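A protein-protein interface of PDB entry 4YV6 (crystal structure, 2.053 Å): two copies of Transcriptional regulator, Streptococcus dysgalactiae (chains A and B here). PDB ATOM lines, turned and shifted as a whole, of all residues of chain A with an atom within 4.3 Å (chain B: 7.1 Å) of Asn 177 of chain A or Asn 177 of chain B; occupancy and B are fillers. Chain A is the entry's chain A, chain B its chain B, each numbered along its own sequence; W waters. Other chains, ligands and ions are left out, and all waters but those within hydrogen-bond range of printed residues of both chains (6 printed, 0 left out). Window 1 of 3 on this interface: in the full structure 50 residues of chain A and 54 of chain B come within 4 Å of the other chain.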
ATOM      1  N   ASP A  60      20.697 -10.585  19.853  1.00  0.00           N
ATOM      2  CA  ASP A  60      20.996  -9.426  19.011  1.00  0.00           C
ATOM      3  C   ASP A  60      21.217  -8.186  19.867  1.00  0.00           C
ATOM      4  O   ASP A  60      22.006  -7.304  19.524  1.00  0.00           O
ATOM      5  CB  ASP A  60      19.859  -9.165  18.018  1.00  0.00           C
ATOM      6  CG  ASP A  60      19.654 -10.310  17.043  1.00  0.00           C
ATOM      7  OD1 ASP A  60      18.936 -11.271  17.392  1.00  0.00           O
ATOM      8  OD2 ASP A  60      20.205 -10.240  15.923  1.00  0.00           O
ATOM      9  N   SER A  64      24.912  -5.959  21.142  1.00  0.00           N
ATOM     10  CA  SER A  64      24.933  -4.504  21.028  1.00  0.00           C
ATOM     11  C   SER A  64      25.445  -3.852  22.311  1.00  0.00           C
ATOM     12  O   SER A  64      26.356  -3.027  22.276  1.00  0.00           O
ATOM     13  CB  SER A  64      23.534  -3.976  20.695  1.00  0.00           C
ATOM     14  OG  SER A  64      23.096  -4.452  19.435  1.00  0.00           O
ATOM     15  N   SER A 174      18.243 -11.859  10.484  1.00  0.00           N
ATOM     16  CA  SER A 174      17.371 -12.162  11.607  1.00  0.00           C
ATOM     17  C   SER A 174      16.057 -11.408  11.462  1.00  0.00           C
ATOM     18  O   SER A 174      16.032 -10.276  10.987  1.00  0.00           O
ATOM     19  CB  SER A 174      18.051 -11.795  12.928  1.00  0.00           C
ATOM     20  OG  SER A 174      17.162 -11.958  14.019  1.00  0.00           O
ATOM     21  N   GLU A 175      14.964 -12.042  11.865  1.00  0.00           N
ATOM     22  CA  GLU A 175      13.673 -11.366  11.884  1.00  0.00           C
ATOM     23  C   GLU A 175      13.677 -10.336  13.007  1.00  0.00           C
ATOM     24  O   GLU A 175      12.972  -9.327  12.947  1.00  0.00           O
ATOM     25  CB  GLU A 175      12.534 -12.370  12.070  1.00  0.00           C
ATOM     26  CG  GLU A 175      11.141 -11.766  11.946  1.00  0.00           C
ATOM     27  CD  GLU A 175      10.882 -11.154  10.580  1.00  0.00           C
ATOM     28  OE1 GLU A 175      11.586 -11.522   9.616  1.00  0.00           O
ATOM     29  OE2 GLU A 175       9.972 -10.304  10.471  1.00  0.00           O
ATOM     30  N   GLN A 176      14.488 -10.600  14.025  1.00  0.00           N
ATOM     31  CA  GLN A 176      14.650  -9.691  15.152  1.00  0.00           C
ATOM     32  C   GLN A 176      15.633  -8.567  14.816  1.00  0.00           C
ATOM     33  O   GLN A 176      15.699  -7.557  15.517  1.00  0.00           O
ATOM     34  CB  GLN A 176      15.128 -10.463  16.383  1.00  0.00           C
ATOM     35  CG  GLN A 176      14.226 -11.634  16.762  1.00  0.00           C
ATOM     36  CD  GLN A 176      14.818 -12.508  17.854  1.00  0.00           C
ATOM     37  OE1 GLN A 176      16.039 -12.600  18.002  1.00  0.00           O
ATOM     38  NE2 GLN A 176      13.952 -13.155  18.627  1.00  0.00           N
ATOM     39  N   ASN A 177      16.391  -8.754  13.738  1.00  0.00           N
ATOM     40  CA  ASN A 177      17.373  -7.770  13.294  1.00  0.00           C
ATOM     41  C   ASN A 177      17.571  -7.845  11.784  1.00  0.00           C
ATOM     42  O   ASN A 177      18.327  -8.682  11.291  1.00  0.00           O
ATOM     43  CB  ASN A 177      18.708  -7.985  14.009  1.00  0.00           C
ATOM     44  CG  ASN A 177      19.777  -7.011  13.554  1.00  0.00           C
ATOM     45  OD1 ASN A 177      19.476  -5.943  13.021  1.00  0.00           O
ATOM     46  ND2 ASN A 177      21.038  -7.375  13.764  1.00  0.00           N
ATOM     47  N   LYS A 178      16.897  -6.957  11.059  1.00  0.00           N
ATOM     48  CA  LYS A 178      16.873  -7.010   9.602  1.00  0.00           C
ATOM     49  C   LYS A 178      17.946  -6.131   8.973  1.00  0.00           C
ATOM     50  O   LYS A 178      17.801  -5.694   7.831  1.00  0.00           O
ATOM     51  CB  LYS A 178      15.494  -6.592   9.080  1.00  0.00           C
ATOM     52  CG  LYS A 178      14.347  -7.422   9.633  1.00  0.00           C
ATOM     53  CD  LYS A 178      13.036  -7.106   8.920  1.00  0.00           C
ATOM     54  CE  LYS A 178      11.904  -7.980   9.427  1.00  0.00           C
ATOM     55  NZ  LYS A 178      10.667  -7.829   8.614  1.00  0.00           N
ATOM     56  N   THR A 179      19.019  -5.875   9.719  1.00  0.00           N
ATOM     57  CA  THR A 179      20.125  -5.062   9.225  1.00  0.00           C
ATOM     58  C   THR A 179      20.655  -5.592   7.895  1.00  0.00           C
ATOM     59  O   THR A 179      20.749  -4.846   6.923  1.00  0.00           O
ATOM     60  CB  THR A 179      21.285  -5.009  10.245  1.00  0.00           C
ATOM     61  OG1 THR A 179      20.835  -4.390  11.455  1.00  0.00           O
ATOM     62  CG2 THR A 179      22.467  -4.215   9.692  1.00  0.00           C
ATOM     63  N   ASP B  60      24.876 -13.227  17.246  1.00  0.00           N
ATOM     64  CA  ASP B  60      23.497 -12.932  16.867  1.00  0.00           C
ATOM     65  C   ASP B  60      23.197 -13.404  15.443  1.00  0.00           C
ATOM     66  O   ASP B  60      22.092 -13.870  15.161  1.00  0.00           O
ATOM     67  CB  ASP B  60      23.213 -11.435  17.004  1.00  0.00           C
ATOM     68  CG  ASP B  60      24.114 -10.586  16.134  1.00  0.00           C
ATOM     69  OD1 ASP B  60      25.282 -10.376  16.520  1.00  0.00           O
ATOM     70  OD2 ASP B  60      23.652 -10.120  15.071  1.00  0.00           O
ATOM     71  N   GLU B  61      24.177 -13.286  14.550  1.00  0.00           N
ATOM     72  CA  GLU B  61      24.055 -13.849  13.206  1.00  0.00           C
ATOM     73  C   GLU B  61      23.998 -15.369  13.274  1.00  0.00           C
ATOM     74  O   GLU B  61      23.227 -16.008  12.558  1.00  0.00           O
ATOM     75  CB  GLU B  61      25.227 -13.424  12.316  1.00  0.00           C
ATOM     76  CG  GLU B  61      25.112 -12.031  11.728  1.00  0.00           C
ATOM     77  CD  GLU B  61      26.178 -11.759  10.681  1.00  0.00           C
ATOM     78  OE1 GLU B  61      25.814 -11.515   9.512  1.00  0.00           O
ATOM     79  OE2 GLU B  61      27.381 -11.792  11.026  1.00  0.00           O
ATOM     80  N   SER B  64      20.654 -16.656  14.335  1.00  0.00           N
ATOM     81  CA  SER B  64      19.608 -16.422  13.338  1.00  0.00           C
ATOM     82  C   SER B  64      19.558 -17.581  12.348  1.00  0.00           C
ATOM     83  O   SER B  64      18.480 -18.060  11.997  1.00  0.00           O
ATOM     84  CB  SER B  64      19.834 -15.103  12.599  1.00  0.00           C
ATOM     85  OG  SER B  64      20.991 -15.163  11.787  1.00  0.00           O
ATOM     86  N   PHE B  74       9.446 -12.644  21.695  1.00  0.00           N
ATOM     87  CA  PHE B  74       9.300 -12.349  20.274  1.00  0.00           C
ATOM     88  C   PHE B  74       8.286 -13.284  19.619  1.00  0.00           C
ATOM     89  O   PHE B  74       7.629 -12.913  18.646  1.00  0.00           O
ATOM     90  CB  PHE B  74      10.645 -12.455  19.553  1.00  0.00           C
ATOM     91  CG  PHE B  74      10.609 -11.957  18.135  1.00  0.00           C
ATOM     92  CD1 PHE B  74      10.827 -10.618  17.853  1.00  0.00           C
ATOM     93  CD2 PHE B  74      10.347 -12.823  17.085  1.00  0.00           C
ATOM     94  CE1 PHE B  74      10.793 -10.154  16.550  1.00  0.00           C
ATOM     95  CE2 PHE B  74      10.310 -12.365  15.781  1.00  0.00           C
ATOM     96  CZ  PHE B  74      10.533 -11.028  15.514  1.00  0.00           C
ATOM     97  N   ALA B 172      19.622   1.271  24.703  1.00  0.00           N
ATOM     98  CA  ALA B 172      20.889   0.835  24.124  1.00  0.00           C
ATOM     99  C   ALA B 172      20.740   0.482  22.649  1.00  0.00           C
ATOM    100  O   ALA B 172      19.732  -0.093  22.232  1.00  0.00           O
ATOM    101  CB  ALA B 172      21.438  -0.357  24.895  1.00  0.00           C
ATOM    102  N   TYR B 173      21.758   0.832  21.867  1.00  0.00           N
ATOM    103  CA  TYR B 173      21.814   0.474  20.457  1.00  0.00           C
ATOM    104  C   TYR B 173      23.259   0.491  19.973  1.00  0.00           C
ATOM    105  O   TYR B 173      24.086   1.245  20.488  1.00  0.00           O
ATOM    106  CB  TYR B 173      20.965   1.429  19.613  1.00  0.00           C
ATOM    107  CG  TYR B 173      21.648   2.741  19.294  1.00  0.00           C
ATOM    108  CD1 TYR B 173      21.657   3.783  20.211  1.00  0.00           C
ATOM    109  CD2 TYR B 173      22.280   2.938  18.073  1.00  0.00           C
ATOM    110  CE1 TYR B 173      22.280   4.984  19.923  1.00  0.00           C
ATOM    111  CE2 TYR B 173      22.906   4.136  17.775  1.00  0.00           C
ATOM    112  CZ  TYR B 173      22.902   5.155  18.703  1.00  0.00           C
ATOM    113  OH  TYR B 173      23.521   6.349  18.412  1.00  0.00           O
ATOM    114  N   SER B 174      23.555  -0.350  18.987  1.00  0.00           N
ATOM    115  CA  SER B 174      24.873  -0.379  18.361  1.00  0.00           C
ATOM    116  C   SER B 174      24.773   0.122  16.930  1.00  0.00           C
ATOM    117  O   SER B 174      23.677   0.238  16.375  1.00  0.00           O
ATOM    118  CB  SER B 174      25.457  -1.792  18.383  1.00  0.00           C
ATOM    119  OG  SER B 174      24.705  -2.668  17.562  1.00  0.00           O
ATOM    120  N   GLU B 175      25.920   0.417  16.334  1.00  0.00           N
ATOM    121  CA  GLU B 175      25.958   0.890  14.959  1.00  0.00           C
ATOM    122  C   GLU B 175      25.552  -0.215  13.990  1.00  0.00           C
ATOM    123  O   GLU B 175      25.153   0.058  12.858  1.00  0.00           O
ATOM    124  CB  GLU B 175      27.354   1.416  14.614  1.00  0.00           C
ATOM    125  CG  GLU B 175      27.693   2.746  15.277  1.00  0.00           C
ATOM    126  CD  GLU B 175      26.701   3.845  14.923  1.00  0.00           C
ATOM    127  OE1 GLU B 175      26.190   3.843  13.783  1.00  0.00           O
ATOM    128  OE2 GLU B 175      26.427   4.703  15.789  1.00  0.00           O
ATOM    129  N   GLN B 176      25.651  -1.461  14.445  1.00  0.00           N
ATOM    130  CA  GLN B 176      25.287  -2.615  13.629  1.00  0.00           C
ATOM    131  C   GLN B 176      23.847  -3.059  13.873  1.00  0.00           C
ATOM    132  O   GLN B 176      23.365  -3.991  13.229  1.00  0.00           O
ATOM    133  CB  GLN B 176      26.238  -3.782  13.908  1.00  0.00           C
ATOM    134  CG  GLN B 176      27.662  -3.548  13.418  1.00  0.00           C
ATOM    135  CD  GLN B 176      28.448  -2.586  14.287  1.00  0.00           C
ATOM    136  OE1 GLN B 176      28.331  -2.594  15.513  1.00  0.00           O
ATOM    137  NE2 GLN B 176      29.257  -1.746  13.651  1.00  0.00           N
ATOM    138  N   ASN B 177      23.164  -2.394  14.800  1.00  0.00           N
ATOM    139  CA  ASN B 177      21.789  -2.751  15.138  1.00  0.00           C
ATOM    140  C   ASN B 177      21.011  -1.547  15.661  1.00  0.00           C
ATOM    141  O   ASN B 177      21.030  -1.250  16.855  1.00  0.00           O
ATOM    142  CB  ASN B 177      21.780  -3.883  16.169  1.00  0.00           C
ATOM    143  CG  ASN B 177      20.391  -4.446  16.409  1.00  0.00           C
ATOM    144  OD1 ASN B 177      19.436  -4.094  15.716  1.00  0.00           O
ATOM    145  ND2 ASN B 177      20.277  -5.335  17.389  1.00  0.00           N
ATOM    146  N   LYS B 178      20.322  -0.864  14.750  1.00  0.00           N
ATOM    147  CA  LYS B 178      19.584   0.352  15.079  1.00  0.00           C
ATOM    148  C   LYS B 178      18.129   0.073  15.452  1.00  0.00           C
ATOM    149  O   LYS B 178      17.332   1.003  15.574  1.00  0.00           O
ATOM    150  CB  LYS B 178      19.617   1.324  13.897  1.00  0.00           C
ATOM    151  CG  LYS B 178      21.009   1.689  13.409  1.00  0.00           C
ATOM    152  CD  LYS B 178      21.726   2.606  14.385  1.00  0.00           C
ATOM    153  CE  LYS B 178      23.125   2.941  13.891  1.00  0.00           C
ATOM    154  NZ  LYS B 178      23.127   3.712  12.618  1.00  0.00           N
ATOM    155  N   THR B 179      17.792  -1.203  15.627  1.00  0.00           N
ATOM    156  CA  THR B 179      16.408  -1.622  15.853  1.00  0.00           C
ATOM    157  C   THR B 179      15.735  -0.865  16.997  1.00  0.00           C
ATOM    158  O   THR B 179      14.689  -0.242  16.804  1.00  0.00           O
ATOM    159  CB  THR B 179      16.334  -3.138  16.145  1.00  0.00           C
ATOM    160  OG1 THR B 179      16.842  -3.867  15.022  1.00  0.00           O
ATOM    161  CG2 THR B 179      14.899  -3.581  16.416  1.00  0.00           C
ATOM    162  N   ASN B 180      16.332  -0.917  18.185  1.00  0.00           N
ATOM    163  CA  ASN B 180      15.755  -0.257  19.352  1.00  0.00           C
ATOM    164  C   ASN B 180      15.683   1.256  19.183  1.00  0.00           C
ATOM    165  O   ASN B 180      14.753   1.894  19.668  1.00  0.00           O
ATOM    166  CB  ASN B 180      16.557  -0.596  20.609  1.00  0.00           C
ATOM    167  CG  ASN B 180      16.330  -2.019  21.081  1.00  0.00           C
ATOM    168  OD1 ASN B 180      15.507  -2.746  20.523  1.00  0.00           O
ATOM    169  ND2 ASN B 180      17.070  -2.430  22.108  1.00  0.00           N
ATOM    170  N   LYS B 181      16.662   1.827  18.488  1.00  0.00           N
ATOM    171  CA  LYS B 181      16.716   3.272  18.300  1.00  0.00           C
ATOM    172  C   LYS B 181      15.566   3.757  17.418  1.00  0.00           C
ATOM    173  O   LYS B 181      14.977   4.808  17.669  1.00  0.00           O
ATOM    174  CB  LYS B 181      18.055   3.677  17.686  1.00  0.00           C
ATOM    175  CG  LYS B 181      18.227   5.177  17.518  1.00  0.00           C
ATOM    176  CD  LYS B 181      19.636   5.524  17.055  1.00  0.00           C
ATOM    177  CE  LYS B 181      19.813   7.024  16.904  1.00  0.00           C
ATOM    178  NZ  LYS B 181      21.182   7.380  16.430  1.00  0.00           N
HETATM  179  O   HOH W   1      19.688  -4.165  20.126  1.00  0.00           O
HETATM  180  O   HOH W   2      21.445 -12.421  10.680  1.00  0.00           O
HETATM  181  O   HOH W   3      15.234  -5.055  12.945  1.00  0.00           O
HETATM  182  O   HOH W   4      17.735  -6.246  17.217  1.00  0.00           O
HETATM  183  O   HOH W   5      19.483 -13.635  15.944  1.00  0.00           O
HETATM  184  O   HOH W   6      20.731  -1.596  11.960  1.00  0.00           O
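O of Asp 60 of chain A lies within hydrogen-bond range of ND2 of Asn 177 of chain B (3.4 Å).
The side-chain hydroxyl of Ser 64 of chain A sits at hydrogen-bond distance from the side-chain hydroxyl of Ser 174 of chain B (3.0 Å).
The side-chain amide oxygen (OD1) of Asn 177 of chain A sits close to the side-chain amide oxygen (OD1) of Asn 177 of chain B (3.3 Å).
OG1 of Thr 179 of chain A is in hydrogen-bond range of O of Gln 176 of chain B (3.1 Å).
The backbone carbonyl oxygen of Asp 60 of chain A sits at hydrogen-bond distance from the side-chain hydroxyl of Ser 64 of chain A, 3.1 Å away.
The side-chain amide oxygen of Gln 176 of chain A lies close to the side-chain carboxylate of Asp 60 of chain A.
The side-chain carboxylate (OE2) of Glu 175 of chain A lies within salt-bridge range of the side-chain amino group (NZ) of Lys 178 of chain A, 3.2 Å away.
OG1 of Thr 179 of chain A sits at hydrogen-bond distance from OD1 of Asn 177 of chain A (2.6 Å).
OG of Ser 174 of chain B sits at hydrogen-bond distance from N of Asn 177 of chain B (3.2 Å).
OD1 of Asn 177 of chain B is in hydrogen-bond range of OG1 of Thr 179 of chain B (2.7 Å).
Among the printed residues, merely in contact across the chains: Asp 60 of chain A with Asp 60 of chain B (3.4 Å), Ser 64 of chain A with Asn 177 of chain B (3.6 Å), Ser 174 of chain A with Ser 64 of chain B (3.8 Å), Glu 175 of chain A with Phe 74 of chain B (3.7 Å), Gln 176 of chain A with Phe 74 of chain B (3.5 Å), Gln 176 of chain A with Thr 179 of chain B (3.9 Å) and Asn 177 of chain A with Thr 179 of chain B (3.9 Å).
Printed residues of chain B within 4 Å of Gln 176 of chain A: Phe 74 (3.5 Å) and Thr 179 (3.9 Å).
Printed residues of chain B within 4 Å of Asn 177 of chain A: Asn 177 (3.3 Å) and Thr 179 (3.9 Å).
Printed residues of chain A within 4 Å of Ser 64 of chain B: Ser 174 (3.8 Å).
Printed residues of chain A within 4 Å of Ser 174 of chain B: Ser 64 (3.0 Å).
Glu 175 of chain B touches none of the printed residues of chain A.
Of chain A, only Asp 60, Ser 64 and Asn 177 come within 4 Å of Asn 177 of chain B.
The nearest residue of chain A that does not touch Asn 177 of chain B is Thr 179 of chain A (4.1 Å).
The nearest printed residue of chain A that does not touch Ser 64 of chain B is Glu 175 of chain A (5.8 Å).
Of the 8 printed residues of chain A, 7 touch a printed residue of chain B.
Printed residues of chain A that touch a printed residue of chain B: Asp 60, Ser 64, Ser 174, Glu 175, Gln 176, Asn 177 and Thr 179.
Asp 60 of chain A touches Asn 177 of chain B, but with the chains exchanged Asn 177 of chain A does not touch Asp 60 of chain B (4.01 Å).
Ser 64 of chain A touches Asn 177 of chain B, but with the chains exchanged Asn 177 of chain A does not touch Ser 64 of chain B (6.7 Å).
Gln 176 of chain A touches Thr 179 of chain B, and with the chains exchanged Thr 179 of chain A touches Gln 176 of chain B.
Asn 177 of chain A touches Thr 179 of chain B, but with the chains exchanged Thr 179 of chain A does not touch Asn 177 of chain B (4.1 Å).
Water W4 lies within hydrogen-bond range of ND2 of Asn 177 of chain B (2.7 Å), O of Gln 176 of chain A (3.0 Å) and OG1 of Thr 179 of chain B (3.4 Å).
Water W5 lies within hydrogen-bond range of the backbone carbonyl oxygen of Asp 60 of chain B, the side-chain carboxylate of Asp 60 of chain A and the side-chain hydroxyl of Ser 174 of chain A.
Water W6 bridges OG1 of Thr 179 of chain A (2.8 Å) and N of Lys 178 of chain B (2.9 Å).
Water W3 bridges OG1 of Thr 179 of chain B (2.9 Å) and N of Lys 178 of chain A (3.2 Å).
Water W2 lies within hydrogen-bond range of the side-chain hydroxyl of Ser 64 of chain B (3.0 Å) and the backbone NH of Ser 174 of chain A (3.3 Å).
Water W1 bridges ND2 of Asn 177 of chain B and OG of Ser 64 of chain A.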
